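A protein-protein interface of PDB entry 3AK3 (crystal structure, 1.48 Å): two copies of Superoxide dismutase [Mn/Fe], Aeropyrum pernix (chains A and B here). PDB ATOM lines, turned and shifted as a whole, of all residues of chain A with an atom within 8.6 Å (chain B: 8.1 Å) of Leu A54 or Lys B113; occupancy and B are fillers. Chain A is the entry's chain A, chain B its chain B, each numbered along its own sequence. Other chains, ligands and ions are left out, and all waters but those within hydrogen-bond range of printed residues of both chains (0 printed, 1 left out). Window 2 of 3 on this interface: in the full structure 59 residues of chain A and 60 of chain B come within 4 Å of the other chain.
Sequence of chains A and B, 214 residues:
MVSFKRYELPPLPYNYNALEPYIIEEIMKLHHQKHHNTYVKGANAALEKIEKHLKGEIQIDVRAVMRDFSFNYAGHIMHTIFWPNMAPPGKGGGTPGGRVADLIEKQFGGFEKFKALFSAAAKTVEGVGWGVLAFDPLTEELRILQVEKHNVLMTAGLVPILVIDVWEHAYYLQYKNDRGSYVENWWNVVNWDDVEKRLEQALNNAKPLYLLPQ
Hydrophobic or aromatic side chains of chain B that line the printed part of chain A: Phe B108, Leu B117 and Ile B144.
Along chain B the printed residues that touch a printed residue of chain A span positions 105 to 144.
Of the 18 printed residues of chain A, 5 touch a printed residue of chain B.
Hydrophobic or aromatic side chains of chain A within 4 Å of the printed part of chain B: Met A1, Val A2, Ile A50, Leu A54 and Met A66.
Among the printed residues, no Asp or Glu carboxylate lies within 4 Å of a Lys or Arg side-chain nitrogen of the other chain.
Among the printed residues, pairs that only touch across the chains: Met A1 with Glu B105, Met A1 with Lys B106, Met A1 with Phe B108, Met A1 with Gly B109, Met A1 with Lys B113, Ile A50 with Leu B117, Leu A54 with Gln B107, Leu A54 with Phe B108, Met A66 with Leu B117 and Met A66 with Ile B144.
The backbone NH (N) of Val A2 lies within hydrogen-bond range of the backbone carbonyl oxygen (O) of Lys B106, 2.8 Å away.
The side-chain amino group of Lys B113 lies within hydrogen-bond range of the backbone carbonyl oxygen of Leu A54 (2.8 Å).
No position is printed for both chains.
Of chain B, only Gln B107, Phe B108 and Lys B113 come within 4 Å of Leu A54.
Lys B113 touches two residues of chain A.
Of the printed residues of chain B, Val A2 touches Lys B106 (2.8 Å).
Of the printed residues of chain A, Phe B108 touches Met A1 and Leu A54.
Printed residues of chain A within 4 Å of Lys B106: Met A1 (3.5 Å) and Val A2 (2.8 Å).
The nearest residue of chain A that does not touch Lys B113 is Lys A55 (4.6 Å).
The nearest printed residue of chain A that does not touch Gly B109 is Leu A54 (5.5 Å).
O of Ile B104 is in hydrogen-bond range of N of Gly B109 (3.3 Å).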
ATOM      1  N   MET A   1     -17.399 -14.589  33.481  1.00  0.00           N
ATOM      2  CA  MET A   1     -17.812 -13.397  32.688  1.00  0.00           C
ATOM      3  C   MET A   1     -19.188 -13.621  32.067  1.00  0.00           C
ATOM      4  O   MET A   1     -19.505 -14.729  31.618  1.00  0.00           O
ATOM      5  CB  MET A   1     -16.782 -13.090  31.594  1.00  0.00           C
ATOM      6  CG  MET A   1     -16.751 -11.624  31.157  1.00  0.00           C
ATOM      7  SD  MET A   1     -15.716 -11.263  29.707  1.00  0.00           S
ATOM      8  CE  MET A   1     -14.105 -11.868  30.200  1.00  0.00           C
ATOM      9  N   VAL A   2     -20.002 -12.568  32.060  1.00  0.00           N
ATOM     10  CA  VAL A   2     -21.324 -12.600  31.438  1.00  0.00           C
ATOM     11  C   VAL A   2     -21.387 -11.508  30.372  1.00  0.00           C
ATOM     12  O   VAL A   2     -20.994 -10.369  30.625  1.00  0.00           O
ATOM     13  CB  VAL A   2     -22.460 -12.376  32.473  1.00  0.00           C
ATOM     14  CG1 VAL A   2     -23.831 -12.486  31.809  1.00  0.00           C
ATOM     15  CG2 VAL A   2     -22.349 -13.360  33.631  1.00  0.00           C
ATOM     16  N   PHE A   4     -22.535  -8.524  28.139  1.00  0.00           N
ATOM     17  CA  PHE A   4     -23.250  -7.314  28.558  1.00  0.00           C
ATOM     18  C   PHE A   4     -24.734  -7.346  28.208  1.00  0.00           C
ATOM     19  O   PHE A   4     -25.146  -7.971  27.223  1.00  0.00           O
ATOM     20  CB  PHE A   4     -22.599  -6.049  27.973  1.00  0.00           C
ATOM     21  CG  PHE A   4     -22.764  -5.893  26.477  1.00  0.00           C
ATOM     22  CD1 PHE A   4     -21.925  -6.569  25.589  1.00  0.00           C
ATOM     23  CD2 PHE A   4     -23.737  -5.043  25.956  1.00  0.00           C
ATOM     24  CE1 PHE A   4     -22.062  -6.415  24.215  1.00  0.00           C
ATOM     25  CE2 PHE A   4     -23.880  -4.884  24.578  1.00  0.00           C
ATOM     26  CZ  PHE A   4     -23.038  -5.573  23.703  1.00  0.00           C
ATOM     27  N   LEU A  47     -19.768  -1.655  23.183  1.00  0.00           N
ATOM     28  CA  LEU A  47     -19.668  -2.644  24.248  1.00  0.00           C
ATOM     29  C   LEU A  47     -19.175  -4.000  23.735  1.00  0.00           C
ATOM     30  O   LEU A  47     -18.492  -4.738  24.457  1.00  0.00           O
ATOM     31  CB  LEU A  47     -21.001  -2.769  24.987  1.00  0.00           C
ATOM     32  CG  LEU A  47     -21.265  -1.642  25.996  1.00  0.00           C
ATOM     33  CD1 LEU A  47     -22.624  -1.802  26.633  1.00  0.00           C
ATOM     34  CD2 LEU A  47     -20.202  -1.600  27.087  1.00  0.00           C
ATOM     35  N   GLU A  48     -19.512  -4.310  22.486  1.00  0.00           N
ATOM     36  CA  GLU A  48     -19.109  -5.573  21.884  1.00  0.00           C
ATOM     37  C   GLU A  48     -17.602  -5.537  21.663  1.00  0.00           C
ATOM     38  O   GLU A  48     -16.916  -6.533  21.909  1.00  0.00           O
ATOM     39  CB  GLU A  48     -19.853  -5.812  20.576  1.00  0.00           C
ATOM     40  CG  GLU A  48     -19.478  -7.087  19.865  1.00  0.00           C
ATOM     41  CD  GLU A  48     -20.295  -7.304  18.619  1.00  0.00           C
ATOM     42  OE1 GLU A  48     -20.649  -6.300  17.960  1.00  0.00           O
ATOM     43  OE2 GLU A  48     -20.587  -8.478  18.301  1.00  0.00           O
ATOM     44  N   LYS A  49     -17.087  -4.382  21.239  1.00  0.00           N
ATOM     45  CA  LYS A  49     -15.639  -4.217  21.075  1.00  0.00           C
ATOM     46  C   LYS A  49     -14.909  -4.397  22.393  1.00  0.00           C
ATOM     47  O   LYS A  49     -13.889  -5.088  22.469  1.00  0.00           O
ATOM     48  CB  LYS A  49     -15.317  -2.858  20.459  1.00  0.00           C
ATOM     49  CG  LYS A  49     -15.738  -2.772  19.018  1.00  0.00           C
ATOM     50  CD  LYS A  49     -15.554  -1.392  18.442  1.00  0.00           C
ATOM     51  CE  LYS A  49     -16.283  -1.289  17.121  1.00  0.00           C
ATOM     52  NZ  LYS A  49     -16.158   0.084  16.556  1.00  0.00           N
ATOM     53  N   ILE A  50     -15.451  -3.800  23.445  1.00  0.00           N
ATOM     54  CA  ILE A  50     -14.900  -3.981  24.779  1.00  0.00           C
ATOM     55  C   ILE A  50     -14.916  -5.461  25.177  1.00  0.00           C
ATOM     56  O   ILE A  50     -13.905  -5.984  25.657  1.00  0.00           O
ATOM     57  CB  ILE A  50     -15.617  -3.096  25.822  1.00  0.00           C
ATOM     58  CG1 ILE A  50     -15.428  -1.621  25.446  1.00  0.00           C
ATOM     59  CG2 ILE A  50     -15.057  -3.358  27.221  1.00  0.00           C
ATOM     60  CD1 ILE A  50     -15.954  -0.604  26.455  1.00  0.00           C
ATOM     61  N   GLU A  51     -16.036  -6.143  24.940  1.00  0.00           N
ATOM     62  CA  GLU A  51     -16.139  -7.571  25.250  1.00  0.00           C
ATOM     63  C   GLU A  51     -15.079  -8.385  24.499  1.00  0.00           C
ATOM     64  O   GLU A  51     -14.359  -9.179  25.106  1.00  0.00           O
ATOM     65  CB  GLU A  51     -17.545  -8.090  24.948  1.00  0.00           C
ATOM     66  CG  GLU A  51     -17.705  -9.590  25.081  1.00  0.00           C
ATOM     67  CD  GLU A  51     -19.142 -10.028  24.907  1.00  0.00           C
ATOM     68  OE1 GLU A  51     -19.783 -10.329  25.929  1.00  0.00           O
ATOM     69  OE2 GLU A  51     -19.635 -10.056  23.758  1.00  0.00           O
ATOM     70  N   LYS A  52     -14.972  -8.168  23.191  1.00  0.00           N
ATOM     71  CA  LYS A  52     -13.998  -8.915  22.377  1.00  0.00           C
ATOM     72  C   LYS A  52     -12.569  -8.619  22.817  1.00  0.00           C
ATOM     73  O   LYS A  52     -11.711  -9.508  22.793  1.00  0.00           O
ATOM     74  CB  LYS A  52     -14.163  -8.602  20.896  1.00  0.00           C
ATOM     75  CG  LYS A  52     -15.399  -9.195  20.264  1.00  0.00           C
ATOM     76  CD  LYS A  52     -15.444  -8.899  18.772  1.00  0.00           C
ATOM     77  CE  LYS A  52     -16.813  -9.207  18.188  1.00  0.00           C
ATOM     78  NZ  LYS A  52     -16.853  -8.942  16.721  1.00  0.00           N
ATOM     79  N   HIS A  53     -12.307  -7.370  23.201  1.00  0.00           N
ATOM     80  CA  HIS A  53     -11.022  -6.994  23.789  1.00  0.00           C
ATOM     81  C   HIS A  53     -10.744  -7.811  25.050  1.00  0.00           C
ATOM     82  O   HIS A  53      -9.669  -8.393  25.198  1.00  0.00           O
ATOM     83  CB  HIS A  53     -10.986  -5.496  24.118  1.00  0.00           C
ATOM     84  CG  HIS A  53      -9.825  -5.094  24.975  1.00  0.00           C
ATOM     85  ND1 HIS A  53      -8.565  -4.872  24.463  1.00  0.00           N
ATOM     86  CD2 HIS A  53      -9.733  -4.879  26.308  1.00  0.00           C
ATOM     87  CE1 HIS A  53      -7.747  -4.535  25.445  1.00  0.00           C
ATOM     88  NE2 HIS A  53      -8.431  -4.532  26.575  1.00  0.00           N
ATOM     89  N   LEU A  54     -11.723  -7.859  25.951  1.00  0.00           N
ATOM     90  CA  LEU A  54     -11.584  -8.577  27.220  1.00  0.00           C
ATOM     91  C   LEU A  54     -11.425 -10.089  27.040  1.00  0.00           C
ATOM     92  O   LEU A  54     -10.812 -10.759  27.872  1.00  0.00           O
ATOM     93  CB  LEU A  54     -12.777  -8.272  28.135  1.00  0.00           C
ATOM     94  CG  LEU A  54     -12.862  -6.843  28.681  1.00  0.00           C
ATOM     95  CD1 LEU A  54     -14.247  -6.601  29.249  1.00  0.00           C
ATOM     96  CD2 LEU A  54     -11.787  -6.566  29.734  1.00  0.00           C
ATOM     97  N   LYS A  55     -11.970 -10.611  25.948  1.00  0.00           N
ATOM     98  CA  LYS A  55     -11.872 -12.037  25.630  1.00  0.00           C
ATOM     99  C   LYS A  55     -10.575 -12.376  24.888  1.00  0.00           C
ATOM    100  O   LYS A  55     -10.327 -13.543  24.555  1.00  0.00           O
ATOM    101  CB  LYS A  55     -13.090 -12.485  24.818  1.00  0.00           C
ATOM    102  CG  LYS A  55     -14.367 -12.590  25.635  1.00  0.00           C
ATOM    103  CD  LYS A  55     -15.545 -12.997  24.780  1.00  0.00           C
ATOM    104  CE  LYS A  55     -16.765 -13.255  25.645  1.00  0.00           C
ATOM    105  NZ  LYS A  55     -17.998 -13.489  24.840  1.00  0.00           N
ATOM    106  N   GLY A  56      -9.754 -11.357  24.643  1.00  0.00           N
ATOM    107  CA  GLY A  56      -8.473 -11.527  23.957  1.00  0.00           C
ATOM    108  C   GLY A  56      -8.630 -11.848  22.484  1.00  0.00           C
ATOM    109  O   GLY A  56      -7.785 -12.529  21.898  1.00  0.00           O
ATOM    110  N   GLU A  57      -9.701 -11.345  21.877  1.00  0.00           N
ATOM    111  CA  GLU A  57     -10.031 -11.668  20.493  1.00  0.00           C
ATOM    112  C   GLU A  57      -9.665 -10.580  19.484  1.00  0.00           C
ATOM    113  O   GLU A  57      -9.435 -10.874  18.301  1.00  0.00           O
ATOM    114  CB  GLU A  57     -11.515 -12.000  20.372  1.00  0.00           C
ATOM    115  CG  GLU A  57     -11.921 -13.270  21.104  1.00  0.00           C
ATOM    116  CD  GLU A  57     -13.422 -13.484  21.127  1.00  0.00           C
ATOM    117  OE1 GLU A  57     -14.152 -12.714  20.459  1.00  0.00           O
ATOM    118  OE2 GLU A  57     -13.869 -14.430  21.811  1.00  0.00           O
ATOM    119  N   ILE A  58      -9.637  -9.327  19.938  1.00  0.00           N
ATOM    120  CA  ILE A  58      -9.299  -8.195  19.073  1.00  0.00           C
ATOM    121  C   ILE A  58      -8.431  -7.168  19.773  1.00  0.00           C
ATOM    122  O   ILE A  58      -8.307  -7.175  20.999  1.00  0.00           O
ATOM    123  CB  ILE A  58     -10.553  -7.446  18.508  1.00  0.00           C
ATOM    124  CG1 ILE A  58     -11.317  -6.705  19.621  1.00  0.00           C
ATOM    125  CG2 ILE A  58     -11.450  -8.375  17.696  1.00  0.00           C
ATOM    126  CD1 ILE A  58     -12.408  -5.772  19.103  1.00  0.00           C
ATOM    127  N   GLN A  59      -7.841  -6.287  18.970  1.00  0.00           N
ATOM    128  CA  GLN A  59      -7.147  -5.110  19.472  1.00  0.00           C
ATOM    129  C   GLN A  59      -8.085  -3.907  19.412  1.00  0.00           C
ATOM    130  O   GLN A  59      -8.746  -3.682  18.389  1.00  0.00           O
ATOM    131  CB  GLN A  59      -5.898  -4.828  18.635  1.00  0.00           C
ATOM    132  CG  GLN A  59      -4.899  -5.981  18.576  1.00  0.00           C
ATOM    133  CD  GLN A  59      -4.283  -6.286  19.921  1.00  0.00           C
ATOM    134  OE1 GLN A  59      -3.806  -5.389  20.617  1.00  0.00           O
ATOM    135  NE2 GLN A  59      -4.286  -7.556  20.294  1.00  0.00           N
ATOM    136  N   ILE A  60      -8.153  -3.145  20.505  1.00  0.00           N
ATOM    137  CA  ILE A  60      -8.903  -1.883  20.502  1.00  0.00           C
ATOM    138  C   ILE A  60      -8.085  -0.680  20.940  1.00  0.00           C
ATOM    139  O   ILE A  60      -7.115  -0.803  21.690  1.00  0.00           O
ATOM    140  CB  ILE A  60     -10.234  -1.928  21.332  1.00  0.00           C
ATOM    141  CG1 ILE A  60      -9.980  -2.050  22.844  1.00  0.00           C
ATOM    142  CG2 ILE A  60     -11.170  -3.015  20.820  1.00  0.00           C
ATOM    143  CD1 ILE A  60     -11.229  -1.769  23.704  1.00  0.00           C
ATOM    144  N   MET A  66     -14.231   4.058  24.017  1.00  0.00           N
ATOM    145  CA  MET A  66     -14.959   4.730  25.093  1.00  0.00           C
ATOM    146  C   MET A  66     -15.600   6.049  24.641  1.00  0.00           C
ATOM    147  O   MET A  66     -16.701   6.388  25.093  1.00  0.00           O
ATOM    148  CB  MET A  66     -14.101   4.875  26.348  1.00  0.00           C
ATOM    149  CG  MET A  66     -13.913   3.540  27.001  1.00  0.00           C
ATOM    150  SD  MET A  66     -12.731   3.584  28.331  1.00  0.00           S
ATOM    151  CE  MET A  66     -12.703   1.847  28.775  1.00  0.00           C
ATOM    152  N   ILE B 104     -17.548  -7.099  38.805  1.00  0.00           N
ATOM    153  CA  ILE B 104     -16.275  -7.070  38.082  1.00  0.00           C
ATOM    154  C   ILE B 104     -15.997  -8.408  37.378  1.00  0.00           C
ATOM    155  O   ILE B 104     -15.493  -8.427  36.252  1.00  0.00           O
ATOM    156  CB  ILE B 104     -15.097  -6.612  38.985  1.00  0.00           C
ATOM    157  CG1 ILE B 104     -15.148  -5.086  39.177  1.00  0.00           C
ATOM    158  CG2 ILE B 104     -13.760  -7.006  38.388  1.00  0.00           C
ATOM    159  CD1 ILE B 104     -14.132  -4.545  40.177  1.00  0.00           C
ATOM    160  N   GLU B 105     -16.343  -9.514  38.030  1.00  0.00           N
ATOM    161  CA  GLU B 105     -16.225 -10.832  37.400  1.00  0.00           C
ATOM    162  C   GLU B 105     -17.183 -10.945  36.211  1.00  0.00           C
ATOM    163  O   GLU B 105     -16.790 -11.379  35.129  1.00  0.00           O
ATOM    164  CB  GLU B 105     -16.483 -11.949  38.421  1.00  0.00           C
ATOM    165  CG  GLU B 105     -16.322 -13.381  37.874  1.00  0.00           C
ATOM    166  CD  GLU B 105     -14.877 -13.770  37.576  1.00  0.00           C
ATOM    167  OE1 GLU B 105     -14.673 -14.658  36.718  1.00  0.00           O
ATOM    168  OE2 GLU B 105     -13.946 -13.205  38.197  1.00  0.00           O
ATOM    169  N   LYS B 106     -18.429 -10.526  36.411  1.00  0.00           N
ATOM    170  CA  LYS B 106     -19.454 -10.588  35.365  1.00  0.00           C
ATOM    171  C   LYS B 106     -19.183  -9.655  34.181  1.00  0.00           C
ATOM    172  O   LYS B 106     -19.276 -10.077  33.025  1.00  0.00           O
ATOM    173  CB  LYS B 106     -20.840 -10.307  35.951  1.00  0.00           C
ATOM    174  CG  LYS B 106     -21.378 -11.413  36.848  1.00  0.00           C
ATOM    175  CD  LYS B 106     -22.681 -10.988  37.501  1.00  0.00           C
ATOM    176  CE  LYS B 106     -23.208 -12.052  38.448  1.00  0.00           C
ATOM    177  NZ  LYS B 106     -24.319 -11.508  39.277  1.00  0.00           N
ATOM    178  N   GLN B 107     -18.854  -8.395  34.466  1.00  0.00           N
ATOM    179  CA  GLN B 107     -18.641  -7.410  33.404  1.00  0.00           C
ATOM    180  C   GLN B 107     -17.270  -7.549  32.728  1.00  0.00           C
ATOM    181  O   GLN B 107     -17.169  -7.453  31.506  1.00  0.00           O
ATOM    182  CB  GLN B 107     -18.877  -5.973  33.910  1.00  0.00           C
ATOM    183  CG  GLN B 107     -20.324  -5.445  33.756  1.00  0.00           C
ATOM    184  CD  GLN B 107     -21.246  -5.877  34.887  1.00  0.00           C
ATOM    185  OE1 GLN B 107     -21.858  -6.959  34.847  1.00  0.00           O
ATOM    186  NE2 GLN B 107     -21.357  -5.038  35.903  1.00  0.00           N
ATOM    187  N   PHE B 108     -16.224  -7.808  33.511  1.00  0.00           N
ATOM    188  CA  PHE B 108     -14.857  -7.694  32.984  1.00  0.00           C
ATOM    189  C   PHE B 108     -14.028  -8.975  32.971  1.00  0.00           C
ATOM    190  O   PHE B 108     -12.914  -8.968  32.461  1.00  0.00           O
ATOM    191  CB  PHE B 108     -14.086  -6.574  33.703  1.00  0.00           C
ATOM    192  CG  PHE B 108     -14.808  -5.252  33.720  1.00  0.00           C
ATOM    193  CD1 PHE B 108     -14.950  -4.505  32.553  1.00  0.00           C
ATOM    194  CD2 PHE B 108     -15.362  -4.763  34.902  1.00  0.00           C
ATOM    195  CE1 PHE B 108     -15.626  -3.286  32.558  1.00  0.00           C
ATOM    196  CE2 PHE B 108     -16.044  -3.546  34.916  1.00  0.00           C
ATOM    197  CZ  PHE B 108     -16.175  -2.803  33.744  1.00  0.00           C
ATOM    198  N   GLY B 109     -14.562 -10.060  33.523  1.00  0.00           N
ATOM    199  CA  GLY B 109     -13.833 -11.327  33.570  1.00  0.00           C
ATOM    200  C   GLY B 109     -12.788 -11.385  34.668  1.00  0.00           C
ATOM    201  O   GLY B 109     -11.809 -12.128  34.560  1.00  0.00           O
ATOM    202  N   GLY B 110     -12.995 -10.606  35.726  1.00  0.00           N
ATOM    203  CA  GLY B 110     -12.115 -10.644  36.888  1.00  0.00           C
ATOM    204  C   GLY B 110     -11.384  -9.350  37.166  1.00  0.00           C
ATOM    205  O   GLY B 110     -11.389  -8.425  36.336  1.00  0.00           O
ATOM    206  N   PHE B 111     -10.748  -9.286  38.335  1.00  0.00           N
ATOM    207  CA  PHE B 111     -10.090  -8.059  38.774  1.00  0.00           C
ATOM    208  C   PHE B 111      -8.879  -7.665  37.944  1.00  0.00           C
ATOM    209  O   PHE B 111      -8.677  -6.478  37.687  1.00  0.00           O
ATOM    210  CB  PHE B 111      -9.724  -8.074  40.262  1.00  0.00           C
ATOM    211  CG  PHE B 111      -9.095  -6.791  40.724  1.00  0.00           C
ATOM    212  CD1 PHE B 111      -9.875  -5.654  40.922  1.00  0.00           C
ATOM    213  CD2 PHE B 111      -7.718  -6.705  40.926  1.00  0.00           C
ATOM    214  CE1 PHE B 111      -9.300  -4.457  41.332  1.00  0.00           C
ATOM    215  CE2 PHE B 111      -7.131  -5.510  41.337  1.00  0.00           C
ATOM    216  CZ  PHE B 111      -7.926  -4.382  41.540  1.00  0.00           C
ATOM    217  N   GLU B 112      -8.069  -8.643  37.534  1.00  0.00           N
ATOM    218  CA  GLU B 112      -6.880  -8.337  36.739  1.00  0.00           C
ATOM    219  C   GLU B 112      -7.243  -7.756  35.371  1.00  0.00           C
ATOM    220  O   GLU B 112      -6.613  -6.804  34.921  1.00  0.00           O
ATOM    221  CB  GLU B 112      -5.937  -9.546  36.628  1.00  0.00           C
ATOM    222  CG  GLU B 112      -5.165  -9.863  37.928  1.00  0.00           C
ATOM    223  CD  GLU B 112      -4.486  -8.643  38.573  1.00  0.00           C
ATOM    224  OE1 GLU B 112      -4.636  -8.468  39.803  1.00  0.00           O
ATOM    225  OE2 GLU B 112      -3.806  -7.856  37.869  1.00  0.00           O
ATOM    226  N   LYS B 113      -8.278  -8.304  34.736  1.00  0.00           N
ATOM    227  CA  LYS B 113      -8.766  -7.747  33.471  1.00  0.00           C
ATOM    228  C   LYS B 113      -9.369  -6.354  33.668  1.00  0.00           C
ATOM    229  O   LYS B 113      -9.035  -5.425  32.926  1.00  0.00           O
ATOM    230  CB  LYS B 113      -9.757  -8.687  32.784  1.00  0.00           C
ATOM    231  CG  LYS B 113      -9.094  -9.882  32.114  1.00  0.00           C
ATOM    232  CD  LYS B 113      -9.950 -10.431  30.999  1.00  0.00           C
ATOM    233  CE  LYS B 113     -10.447 -11.822  31.301  1.00  0.00           C
ATOM    234  NZ  LYS B 113     -10.714 -12.547  30.027  1.00  0.00           N
ATOM    235  N   PHE B 114     -10.221  -6.210  34.684  1.00  0.00           N
ATOM    236  CA  PHE B 114     -10.727  -4.892  35.068  1.00  0.00           C
ATOM    237  C   PHE B 114      -9.600  -3.870  35.263  1.00  0.00           C
ATOM    238  O   PHE B 114      -9.636  -2.770  34.702  1.00  0.00           O
ATOM    239  CB  PHE B 114     -11.579  -4.972  36.338  1.00  0.00           C
ATOM    240  CG  PHE B 114     -11.728  -3.645  37.050  1.00  0.00           C
ATOM    241  CD1 PHE B 114     -12.606  -2.672  36.568  1.00  0.00           C
ATOM    242  CD2 PHE B 114     -10.969  -3.358  38.184  1.00  0.00           C
ATOM    243  CE1 PHE B 114     -12.732  -1.447  37.217  1.00  0.00           C
ATOM    244  CE2 PHE B 114     -11.088  -2.127  38.837  1.00  0.00           C
ATOM    245  CZ  PHE B 114     -11.967  -1.171  38.352  1.00  0.00           C
ATOM    246  N   LYS B 115      -8.605  -4.227  36.074  1.00  0.00           N
ATOM    247  CA  LYS B 115      -7.521  -3.310  36.407  1.00  0.00           C
ATOM    248  C   LYS B 115      -6.755  -2.874  35.165  1.00  0.00           C
ATOM    249  O   LYS B 115      -6.453  -1.691  35.009  1.00  0.00           O
ATOM    250  CB  LYS B 115      -6.585  -3.931  37.451  1.00  0.00           C
ATOM    251  CG  LYS B 115      -5.423  -3.065  37.848  1.00  0.00           C
ATOM    252  CD  LYS B 115      -4.658  -3.716  39.000  1.00  0.00           C
ATOM    253  CE  LYS B 115      -3.538  -2.824  39.494  1.00  0.00           C
ATOM    254  NZ  LYS B 115      -2.733  -2.255  38.377  1.00  0.00           N
ATOM    255  N   ALA B 116      -6.455  -3.826  34.277  1.00  0.00           N
ATOM    256  CA  ALA B 116      -5.776  -3.509  33.024  1.00  0.00           C
ATOM    257  C   ALA B 116      -6.596  -2.511  32.191  1.00  0.00           C
ATOM    258  O   ALA B 116      -6.055  -1.556  31.665  1.00  0.00           O
ATOM    259  CB  ALA B 116      -5.472  -4.780  32.228  1.00  0.00           C
ATOM    260  N   LEU B 117      -7.902  -2.731  32.112  1.00  0.00           N
ATOM    261  CA  LEU B 117      -8.768  -1.863  31.315  1.00  0.00           C
ATOM    262  C   LEU B 117      -8.966  -0.469  31.923  1.00  0.00           C
ATOM    263  O   LEU B 117      -8.861   0.532  31.216  1.00  0.00           O
ATOM    264  CB  LEU B 117     -10.112  -2.540  31.059  1.00  0.00           C
ATOM    265  CG  LEU B 117     -11.099  -1.782  30.164  1.00  0.00           C
ATOM    266  CD1 LEU B 117     -10.467  -1.447  28.813  1.00  0.00           C
ATOM    267  CD2 LEU B 117     -12.382  -2.567  29.999  1.00  0.00           C
ATOM    268  N   PHE B 118      -9.239  -0.421  33.227  1.00  0.00           N
ATOM    269  CA  PHE B 118      -9.359   0.840  33.948  1.00  0.00           C
ATOM    270  C   PHE B 118      -8.048   1.629  33.853  1.00  0.00           C
ATOM    271  O   PHE B 118      -8.055   2.829  33.551  1.00  0.00           O
ATOM    272  CB  PHE B 118      -9.753   0.599  35.409  1.00  0.00           C
ATOM    273  CG  PHE B 118     -10.102   1.860  36.155  1.00  0.00           C
ATOM    274  CD1 PHE B 118     -11.418   2.297  36.228  1.00  0.00           C
ATOM    275  CD2 PHE B 118      -9.113   2.626  36.759  1.00  0.00           C
ATOM    276  CE1 PHE B 118     -11.740   3.466  36.918  1.00  0.00           C
ATOM    277  CE2 PHE B 118      -9.429   3.795  37.445  1.00  0.00           C
ATOM    278  CZ  PHE B 118     -10.741   4.211  37.525  1.00  0.00           C
ATOM    279  N   SER B 119      -6.917   0.955  34.077  1.00  0.00           N
ATOM    280  CA  SER B 119      -5.613   1.612  33.982  1.00  0.00           C
ATOM    281  C   SER B 119      -5.351   2.164  32.583  1.00  0.00           C
ATOM    282  O   SER B 119      -4.829   3.267  32.434  1.00  0.00           O
ATOM    283  CB  SER B 119      -4.475   0.664  34.380  1.00  0.00           C
ATOM    284  OG  SER B 119      -4.515   0.380  35.761  1.00  0.00           O
ATOM    285  N   ALA B 120      -5.692   1.383  31.555  1.00  0.00           N
ATOM    286  CA  ALA B 120      -5.537   1.855  30.171  1.00  0.00           C
ATOM    287  C   ALA B 120      -6.399   3.084  29.942  1.00  0.00           C
ATOM    288  O   ALA B 120      -5.956   4.047  29.320  1.00  0.00           O
ATOM    289  CB  ALA B 120      -5.912   0.771  29.192  1.00  0.00           C
ATOM    290  N   ILE B 144     -16.863   1.354  32.181  1.00  0.00           N
ATOM    291  CA  ILE B 144     -15.700   2.226  32.294  1.00  0.00           C
ATOM    292  C   ILE B 144     -15.732   3.255  31.170  1.00  0.00           C
ATOM    293  O   ILE B 144     -16.110   2.933  30.037  1.00  0.00           O
ATOM    294  CB  ILE B 144     -14.349   1.427  32.279  1.00  0.00           C
ATOM    295  CG1 ILE B 144     -14.239   0.536  33.524  1.00  0.00           C
ATOM    296  CG2 ILE B 144     -13.131   2.362  32.227  1.00  0.00           C
ATOM    297  CD1 ILE B 144     -13.138  -0.501  33.437  1.00  0.00           C
